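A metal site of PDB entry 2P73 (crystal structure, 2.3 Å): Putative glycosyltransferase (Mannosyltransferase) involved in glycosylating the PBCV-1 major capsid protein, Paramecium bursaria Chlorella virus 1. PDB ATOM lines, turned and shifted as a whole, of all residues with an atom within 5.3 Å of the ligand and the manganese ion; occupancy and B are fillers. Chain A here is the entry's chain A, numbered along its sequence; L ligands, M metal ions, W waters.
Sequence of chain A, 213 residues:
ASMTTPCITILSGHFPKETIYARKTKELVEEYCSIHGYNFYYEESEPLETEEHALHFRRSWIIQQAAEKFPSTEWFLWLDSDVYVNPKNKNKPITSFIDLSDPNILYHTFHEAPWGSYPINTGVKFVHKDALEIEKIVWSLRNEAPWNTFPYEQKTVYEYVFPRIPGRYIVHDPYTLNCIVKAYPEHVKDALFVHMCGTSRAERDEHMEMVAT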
ATOM      1  N   GLY A  13      21.455 -29.460 -13.481  1.00  0.00           N
ATOM      2  CA  GLY A  13      22.843 -29.057 -13.421  1.00  0.00           C
ATOM      3  C   GLY A  13      23.006 -27.738 -14.121  1.00  0.00           C
ATOM      4  O   GLY A  13      22.243 -27.407 -15.036  1.00  0.00           O
ATOM      5  N   HIS A  14      23.994 -26.967 -13.701  1.00  0.00           N
ATOM      6  CA  HIS A  14      24.234 -25.648 -14.270  1.00  0.00           C
ATOM      7  C   HIS A  14      25.678 -25.234 -14.122  1.00  0.00           C
ATOM      8  O   HIS A  14      26.241 -25.290 -13.010  1.00  0.00           O
ATOM      9  CB  HIS A  14      23.321 -24.603 -13.616  1.00  0.00           C
ATOM     10  CG  HIS A  14      23.397 -23.260 -14.263  1.00  0.00           C
ATOM     11  ND1 HIS A  14      22.636 -22.912 -15.356  1.00  0.00           N
ATOM     12  CD2 HIS A  14      24.142 -22.163 -13.958  1.00  0.00           C
ATOM     13  CE1 HIS A  14      22.910 -21.660 -15.704  1.00  0.00           C
ATOM     14  NE2 HIS A  14      23.813 -21.182 -14.874  1.00  0.00           N
ATOM     15  N   PHE A  15      26.269 -24.826 -15.234  1.00  0.00           N
ATOM     16  CA  PHE A  15      27.557 -24.153 -15.252  1.00  0.00           C
ATOM     17  C   PHE A  15      27.352 -22.700 -15.639  1.00  0.00           C
ATOM     18  O   PHE A  15      26.732 -22.417 -16.673  1.00  0.00           O
ATOM     19  CB  PHE A  15      28.541 -24.823 -16.227  1.00  0.00           C
ATOM     20  CG  PHE A  15      29.824 -24.061 -16.398  1.00  0.00           C
ATOM     21  CD1 PHE A  15      29.934 -23.055 -17.356  1.00  0.00           C
ATOM     22  CD2 PHE A  15      30.924 -24.320 -15.571  1.00  0.00           C
ATOM     23  CE1 PHE A  15      31.121 -22.315 -17.506  1.00  0.00           C
ATOM     24  CE2 PHE A  15      32.122 -23.607 -15.706  1.00  0.00           C
ATOM     25  CZ  PHE A  15      32.220 -22.595 -16.685  1.00  0.00           C
ATOM     26  N   PRO A  16      27.888 -21.757 -14.846  1.00  0.00           N
ATOM     27  CA  PRO A  16      28.658 -21.971 -13.618  1.00  0.00           C
ATOM     28  C   PRO A  16      27.787 -22.239 -12.383  1.00  0.00           C
ATOM     29  O   PRO A  16      26.657 -21.731 -12.285  1.00  0.00           O
ATOM     30  CB  PRO A  16      29.423 -20.660 -13.453  1.00  0.00           C
ATOM     31  CG  PRO A  16      28.532 -19.632 -14.040  1.00  0.00           C
ATOM     32  CD  PRO A  16      27.767 -20.315 -15.166  1.00  0.00           C
ATOM     33  N   TYR A  21      20.205 -17.960  -9.425  1.00  0.00           N
ATOM     34  CA  TYR A  21      18.904 -18.509  -9.703  1.00  0.00           C
ATOM     35  C   TYR A  21      18.954 -20.021  -9.843  1.00  0.00           C
ATOM     36  O   TYR A  21      17.986 -20.691  -9.546  1.00  0.00           O
ATOM     37  CB  TYR A  21      18.263 -17.869 -10.952  1.00  0.00           C
ATOM     38  CG  TYR A  21      18.779 -18.374 -12.284  1.00  0.00           C
ATOM     39  CD1 TYR A  21      18.254 -19.539 -12.861  1.00  0.00           C
ATOM     40  CD2 TYR A  21      19.764 -17.689 -12.972  1.00  0.00           C
ATOM     41  CE1 TYR A  21      18.720 -20.027 -14.084  1.00  0.00           C
ATOM     42  CE2 TYR A  21      20.236 -18.154 -14.211  1.00  0.00           C
ATOM     43  CZ  TYR A  21      19.706 -19.320 -14.752  1.00  0.00           C
ATOM     44  OH  TYR A  21      20.173 -19.764 -15.964  1.00  0.00           O
ATOM     45  N   LEU A  55      27.114 -27.008 -23.394  1.00  0.00           N
ATOM     46  CA  LEU A  55      26.364 -26.884 -22.143  1.00  0.00           C
ATOM     47  C   LEU A  55      24.901 -27.295 -22.334  1.00  0.00           C
ATOM     48  O   LEU A  55      24.309 -27.922 -21.452  1.00  0.00           O
ATOM     49  CB  LEU A  55      26.462 -25.465 -21.575  1.00  0.00           C
ATOM     50  CG  LEU A  55      27.865 -24.932 -21.231  1.00  0.00           C
ATOM     51  CD1 LEU A  55      27.765 -23.453 -20.916  1.00  0.00           C
ATOM     52  CD2 LEU A  55      28.500 -25.682 -20.068  1.00  0.00           C
ATOM     53  N   HIS A  56      24.328 -26.958 -23.487  1.00  0.00           N
ATOM     54  CA  HIS A  56      22.971 -27.357 -23.798  1.00  0.00           C
ATOM     55  C   HIS A  56      22.812 -28.851 -24.040  1.00  0.00           C
ATOM     56  O   HIS A  56      21.760 -29.391 -23.766  1.00  0.00           O
ATOM     57  CB  HIS A  56      22.444 -26.581 -24.997  1.00  0.00           C
ATOM     58  CG  HIS A  56      21.945 -25.219 -24.646  1.00  0.00           C
ATOM     59  ND1 HIS A  56      20.614 -24.860 -24.713  1.00  0.00           N
ATOM     60  CD2 HIS A  56      22.608 -24.115 -24.209  1.00  0.00           C
ATOM     61  CE1 HIS A  56      20.484 -23.592 -24.371  1.00  0.00           C
ATOM     62  NE2 HIS A  56      21.677 -23.112 -24.055  1.00  0.00           N
ATOM     63  N   ARG A  59      22.891 -32.252 -20.625  1.00  0.00           N
ATOM     64  CA  ARG A  59      21.837 -33.059 -20.026  1.00  0.00           C
ATOM     65  C   ARG A  59      21.879 -34.510 -20.473  1.00  0.00           C
ATOM     66  O   ARG A  59      21.389 -35.381 -19.755  1.00  0.00           O
ATOM     67  CB  ARG A  59      20.477 -32.453 -20.330  1.00  0.00           C
ATOM     68  CG  ARG A  59      19.879 -32.746 -21.720  1.00  0.00           C
ATOM     69  CD  ARG A  59      18.730 -31.767 -21.977  1.00  0.00           C
ATOM     70  NE  ARG A  59      19.259 -30.432 -22.147  1.00  0.00           N
ATOM     71  CZ  ARG A  59      18.545 -29.306 -22.232  1.00  0.00           C
ATOM     72  NH1 ARG A  59      17.225 -29.331 -22.138  1.00  0.00           N
ATOM     73  NH2 ARG A  59      19.169 -28.160 -22.411  1.00  0.00           N
ATOM     74  N   TRP A  78      14.612 -34.706 -16.685  1.00  0.00           N
ATOM     75  CA  TRP A  78      15.451 -33.547 -16.828  1.00  0.00           C
ATOM     76  C   TRP A  78      14.627 -32.283 -16.651  1.00  0.00           C
ATOM     77  O   TRP A  78      13.573 -32.130 -17.270  1.00  0.00           O
ATOM     78  CB  TRP A  78      16.142 -33.505 -18.204  1.00  0.00           C
ATOM     79  CG  TRP A  78      16.874 -32.194 -18.370  1.00  0.00           C
ATOM     80  CD1 TRP A  78      16.429 -31.066 -19.053  1.00  0.00           C
ATOM     81  CD2 TRP A  78      18.147 -31.849 -17.825  1.00  0.00           C
ATOM     82  NE1 TRP A  78      17.371 -30.066 -18.968  1.00  0.00           N
ATOM     83  CE2 TRP A  78      18.425 -30.512 -18.214  1.00  0.00           C
ATOM     84  CE3 TRP A  78      19.093 -32.544 -17.052  1.00  0.00           C
ATOM     85  CZ2 TRP A  78      19.616 -29.862 -17.842  1.00  0.00           C
ATOM     86  CZ3 TRP A  78      20.273 -31.887 -16.701  1.00  0.00           C
ATOM     87  CH2 TRP A  78      20.527 -30.570 -17.101  1.00  0.00           C
ATOM     88  N   LEU A  79      15.102 -31.423 -15.758  1.00  0.00           N
ATOM     89  CA  LEU A  79      14.585 -30.073 -15.597  1.00  0.00           C
ATOM     90  C   LEU A  79      15.728 -29.106 -15.777  1.00  0.00           C
ATOM     91  O   LEU A  79      16.793 -29.245 -15.159  1.00  0.00           O
ATOM     92  CB  LEU A  79      13.997 -29.867 -14.203  1.00  0.00           C
ATOM     93  CG  LEU A  79      12.883 -30.783 -13.708  1.00  0.00           C
ATOM     94  CD1 LEU A  79      12.541 -30.437 -12.287  1.00  0.00           C
ATOM     95  CD2 LEU A  79      11.671 -30.714 -14.611  1.00  0.00           C
ATOM     96  N   ASP A  80      15.521 -28.144 -16.664  1.00  0.00           N
ATOM     97  CA  ASP A  80      16.471 -27.075 -16.845  1.00  0.00           C
ATOM     98  C   ASP A  80      16.670 -26.341 -15.525  1.00  0.00           C
ATOM     99  O   ASP A  80      15.745 -26.259 -14.694  1.00  0.00           O
ATOM    100  CB  ASP A  80      15.968 -26.094 -17.878  1.00  0.00           C
ATOM    101  CG  ASP A  80      16.423 -26.423 -19.307  1.00  0.00           C
ATOM    102  OD1 ASP A  80      17.138 -27.408 -19.541  1.00  0.00           O
ATOM    103  OD2 ASP A  80      16.063 -25.675 -20.217  1.00  0.00           O
ATOM    104  N   SER A  81      17.872 -25.788 -15.354  1.00  0.00           N
ATOM    105  CA  SER A  81      18.230 -24.951 -14.233  1.00  0.00           C
ATOM    106  C   SER A  81      17.374 -23.698 -14.033  1.00  0.00           C
ATOM    107  O   SER A  81      17.434 -23.073 -12.961  1.00  0.00           O
ATOM    108  CB  SER A  81      19.712 -24.552 -14.334  1.00  0.00           C
ATOM    109  OG  SER A  81      19.959 -23.844 -15.533  1.00  0.00           O
ATOM    110  N   ASP A  82      16.586 -23.314 -15.033  1.00  0.00           N
ATOM    111  CA  ASP A  82      15.656 -22.183 -14.872  1.00  0.00           C
ATOM    112  C   ASP A  82      14.207 -22.656 -14.776  1.00  0.00           C
ATOM    113  O   ASP A  82      13.269 -21.901 -15.064  1.00  0.00           O
ATOM    114  CB  ASP A  82      15.828 -21.181 -16.018  1.00  0.00           C
ATOM    115  CG  ASP A  82      15.654 -21.823 -17.372  1.00  0.00           C
ATOM    116  OD1 ASP A  82      15.805 -23.055 -17.475  1.00  0.00           O
ATOM    117  OD2 ASP A  82      15.354 -21.109 -18.348  1.00  0.00           O
ATOM    118  N   VAL A  83      14.047 -23.930 -14.419  1.00  0.00           N
ATOM    119  CA  VAL A  83      12.750 -24.492 -14.116  1.00  0.00           C
ATOM    120  C   VAL A  83      12.688 -24.713 -12.597  1.00  0.00           C
ATOM    121  O   VAL A  83      13.594 -25.332 -12.010  1.00  0.00           O
ATOM    122  CB  VAL A  83      12.520 -25.865 -14.820  1.00  0.00           C
ATOM    123  CG1 VAL A  83      11.205 -26.493 -14.363  1.00  0.00           C
ATOM    124  CG2 VAL A  83      12.507 -25.735 -16.358  1.00  0.00           C
ATOM    125  N   GLY A 123      13.256 -28.470 -22.031  1.00  0.00           N
ATOM    126  CA  GLY A 123      13.595 -27.983 -20.685  1.00  0.00           C
ATOM    127  C   GLY A 123      12.989 -28.820 -19.565  1.00  0.00           C
ATOM    128  O   GLY A 123      13.452 -28.783 -18.445  1.00  0.00           O
ATOM    129  N   HIS A 195       8.842 -22.667 -16.167  1.00  0.00           N
ATOM    130  CA  HIS A 195      10.093 -22.506 -16.944  1.00  0.00           C
ATOM    131  C   HIS A 195      10.312 -21.029 -17.266  1.00  0.00           C
ATOM    132  O   HIS A 195       9.494 -20.425 -17.957  1.00  0.00           O
ATOM    133  CB  HIS A 195      10.010 -23.274 -18.270  1.00  0.00           C
ATOM    134  CG  HIS A 195      11.323 -23.450 -18.977  1.00  0.00           C
ATOM    135  ND1 HIS A 195      11.448 -24.286 -20.070  1.00  0.00           N
ATOM    136  CD2 HIS A 195      12.568 -22.944 -18.757  1.00  0.00           C
ATOM    137  CE1 HIS A 195      12.706 -24.282 -20.485  1.00  0.00           C
ATOM    138  NE2 HIS A 195      13.410 -23.483 -19.709  1.00  0.00           N
ATOM    139  N   MET A 196      11.413 -20.481 -16.770  1.00  0.00           N
ATOM    140  CA  MET A 196      11.771 -19.093 -17.066  1.00  0.00           C
ATOM    141  C   MET A 196      12.564 -19.022 -18.351  1.00  0.00           C
ATOM    142  O   MET A 196      13.615 -18.391 -18.417  1.00  0.00           O
ATOM    143  CB  MET A 196      12.605 -18.503 -15.947  1.00  0.00           C
ATOM    144  CG  MET A 196      11.923 -18.468 -14.596  1.00  0.00           C
ATOM    145  SD  MET A 196      13.058 -17.833 -13.362  1.00  0.00           S
ATOM    146  CE  MET A 196      14.257 -19.158 -13.232  1.00  0.00           C
ATOM    147  N   CYS A 197      12.055 -19.687 -19.380  1.00  0.00           N
ATOM    148  CA  CYS A 197      12.729 -19.881 -20.672  1.00  0.00           C
ATOM    149  C   CYS A 197      12.990 -18.584 -21.469  1.00  0.00           C
ATOM    150  O   CYS A 197      12.103 -17.721 -21.581  1.00  0.00           O
ATOM    151  CB  CYS A 197      11.893 -20.834 -21.504  1.00  0.00           C
ATOM    152  SG  CYS A 197      12.485 -21.047 -23.174  1.00  0.00           S
ATOM    153  N   GLY A 198      14.189 -18.488 -22.042  1.00  0.00           N
ATOM    154  CA  GLY A 198      14.535 -17.376 -22.948  1.00  0.00           C
ATOM    155  C   GLY A 198      14.620 -15.992 -22.320  1.00  0.00           C
ATOM    156  O   GLY A 198      14.238 -14.989 -22.944  1.00  0.00           O
ATOM    157  N   THR A 199      15.108 -15.954 -21.075  1.00  0.00           N
ATOM    158  CA  THR A 199      15.343 -14.716 -20.321  1.00  0.00           C
ATOM    159  C   THR A 199      16.779 -14.738 -19.802  1.00  0.00           C
ATOM    160  O   THR A 199      17.407 -15.799 -19.758  1.00  0.00           O
ATOM    161  CB  THR A 199      14.390 -14.579 -19.115  1.00  0.00           C
ATOM    162  OG1 THR A 199      14.351 -15.823 -18.412  1.00  0.00           O
ATOM    163  CG2 THR A 199      12.973 -14.209 -19.567  1.00  0.00           C
ATOM    164  N   ARG A 204      16.273 -13.764 -14.544  1.00  0.00           N
ATOM    165  CA  ARG A 204      15.977 -14.990 -13.798  1.00  0.00           C
ATOM    166  C   ARG A 204      16.299 -14.855 -12.307  1.00  0.00           C
ATOM    167  O   ARG A 204      15.546 -15.326 -11.451  1.00  0.00           O
ATOM    168  CB  ARG A 204      16.709 -16.193 -14.406  1.00  0.00           C
ATOM    169  CG  ARG A 204      16.201 -16.592 -15.788  1.00  0.00           C
ATOM    170  CD  ARG A 204      17.100 -17.601 -16.472  1.00  0.00           C
ATOM    171  NE  ARG A 204      16.570 -18.027 -17.773  1.00  0.00           N
ATOM    172  CZ  ARG A 204      17.280 -18.674 -18.691  1.00  0.00           C
ATOM    173  NH1 ARG A 204      18.541 -18.989 -18.459  1.00  0.00           N
ATOM    174  NH2 ARG A 204      16.719 -18.979 -19.855  1.00  0.00           N
HETATM  175  N1  LIG L   1      23.250 -24.152 -19.429  1.00  0.00           N
HETATM  176  C1  LIG L   1      24.318 -23.923 -18.568  1.00  0.00           C
HETATM  177  N2  LIG L   1      24.905 -22.687 -18.516  1.00  0.00           N
HETATM  178  C2  LIG L   1      24.405 -21.656 -19.283  1.00  0.00           C
HETATM  179  C3  LIG L   1      23.324 -21.890 -20.143  1.00  0.00           C
HETATM  180  C4  LIG L   1      22.949 -23.216 -20.387  1.00  0.00           C
HETATM  181  O1  LIG L   1      24.808 -24.791 -17.872  1.00  0.00           O
HETATM  182  O2  LIG L   1      24.961 -20.557 -19.186  1.00  0.00           O
HETATM  183  C5  LIG L   1      22.647 -25.509 -19.460  1.00  0.00           C
HETATM  184  C6  LIG L   1      21.850 -25.655 -18.186  1.00  0.00           C
HETATM  185  O3  LIG L   1      22.087 -26.956 -17.666  1.00  0.00           O
HETATM  186  C7  LIG L   1      20.409 -25.452 -18.621  1.00  0.00           C
HETATM  187  C8  LIG L   1      20.409 -25.803 -20.114  1.00  0.00           C
HETATM  188  O4  LIG L   1      21.763 -25.692 -20.554  1.00  0.00           O
HETATM  189  O5  LIG L   1      19.545 -26.272 -17.855  1.00  0.00           O
HETATM  190  C9  LIG L   1      19.545 -24.891 -20.974  1.00  0.00           C
HETATM  191  O6  LIG L   1      19.901 -23.551 -20.729  1.00  0.00           O
HETATM  192  P1  LIG L   1      18.774 -22.419 -20.705  1.00  0.00           P
HETATM  193  O7  LIG L   1      17.685 -22.793 -19.770  1.00  0.00           O
HETATM  194  O8  LIG L   1      19.292 -21.084 -20.420  1.00  0.00           O
HETATM  195  O9  LIG L   1      18.121 -22.489 -22.187  1.00  0.00           O
HETATM  196  P2  LIG L   1      16.696 -21.844 -22.575  1.00  0.00           P
HETATM  197  O10 LIG L   1      15.535 -22.529 -21.940  1.00  0.00           O
HETATM  198  O11 LIG L   1      16.638 -20.431 -22.111  1.00  0.00           O
HETATM  199  O12 LIG L   1      16.505 -21.944 -24.055  1.00  0.00           O
HETATM  200 MN    MN M   1      15.512 -23.384 -19.747  1.00  0.00          MN
HETATM  201  O   HOH W   1      22.028 -29.077 -20.606  1.00  0.00           O
HETATM  202  O   HOH W   2      19.180 -22.019 -17.025  1.00  0.00           O
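An oxygen (O1) of the ligand sits at hydrogen-bond distance from the backbone NH (N) of Phe 15, 3.0 Å away.
The guanidinium group of Arg 204 is in salt-bridge range of an oxygen (O11) of the ligand, at 2.7 Å.
O11 of the ligand is in hydrogen-bond range of N of Gly 198.
N2 of the ligand sits at hydrogen-bond distance from O of Phe 15, 2.6 Å away.
O3 of the ligand is in hydrogen-bond range of O of Gly 13.
O5 of the ligand lies within hydrogen-bond range of OG of Ser 81, at 3.4 Å.
The backbone NH (N) of Ser 81 sits at hydrogen-bond distance from an oxygen (O5) of the ligand (3.0 Å).
An oxygen (O10) of the ligand lies close to the side-chain sulfur (SG) of Cys 197, 3.6 Å away.
Of the 21 residues printed, 3 come within 4 Å of the manganese ion.
Along chain A the residues within 4 Å of the manganese ion span positions 80 to 195.
OH of Tyr 21 sits at hydrogen-bond distance from NH1 of Arg 204.
The indole nitrogen of Trp 78 is in hydrogen-bond range of the side-chain carboxylate of Asp 80 (2.7 Å).
A ring nitrogen (ND1) of His 14 lies within hydrogen-bond range of the side-chain hydroxyl (OG) of Ser 81.
The guanidinium group (NE) of Arg 204 lies close to the backbone carbonyl oxygen (O) of Thr 199, at 3.1 Å.
NE of Arg 204 is in hydrogen-bond range of O of Met 196 (3.0 Å).
The backbone carbonyl oxygen of Asp 82 sits at hydrogen-bond distance from the backbone NH of Met 196, 2.9 Å away.
N of Asp 80 is in hydrogen-bond range of O of Gly 123, at 2.8 Å.
The backbone carbonyl oxygen (O) of His 56 lies within hydrogen-bond range of the guanidinium group (NE) of Arg 59, 3.2 Å away.
His 14 touches the ligand (CE1 to N2, 3.6 Å).
Leu 55 touches the ligand (O to O4, 3.5 Å).
CE1 of His 56 touches O9 of the ligand, 3.4 Å away.
Arg 59 touches the ligand (NH2 to C8, 3.5 Å).
CZ2 of Trp 78 touches O5 of the ligand, 3.6 Å away.
Hydrophobic or aromatic side chains within 4 Å of the ligand: His 14, Leu 55, His 56, Trp 78 and His 195.
The nearest printed residue that does not touch the ligand is Tyr 21 (4.7 Å).
The manganese ion is bound by NE2 of His 195 (2.1 Å).
The manganese ion is bound by an oxygen (O7) of the ligand, 2.3 Å away.
The manganese ion is bound by OD1 of Asp 82, at 2.3 Å.
The manganese ion is bound by O10 of the ligand, at 2.4 Å.
The side-chain carboxylate (OD2) of Asp 80 binds the manganese ion (2.4 Å).
OD2 of Asp 82 binds the manganese ion.
The manganese ion has six donor atoms within binding distance.
Water W2 lies within hydrogen-bond range of OG of Ser 81, OH of Tyr 21 and NH1 of Arg 204.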
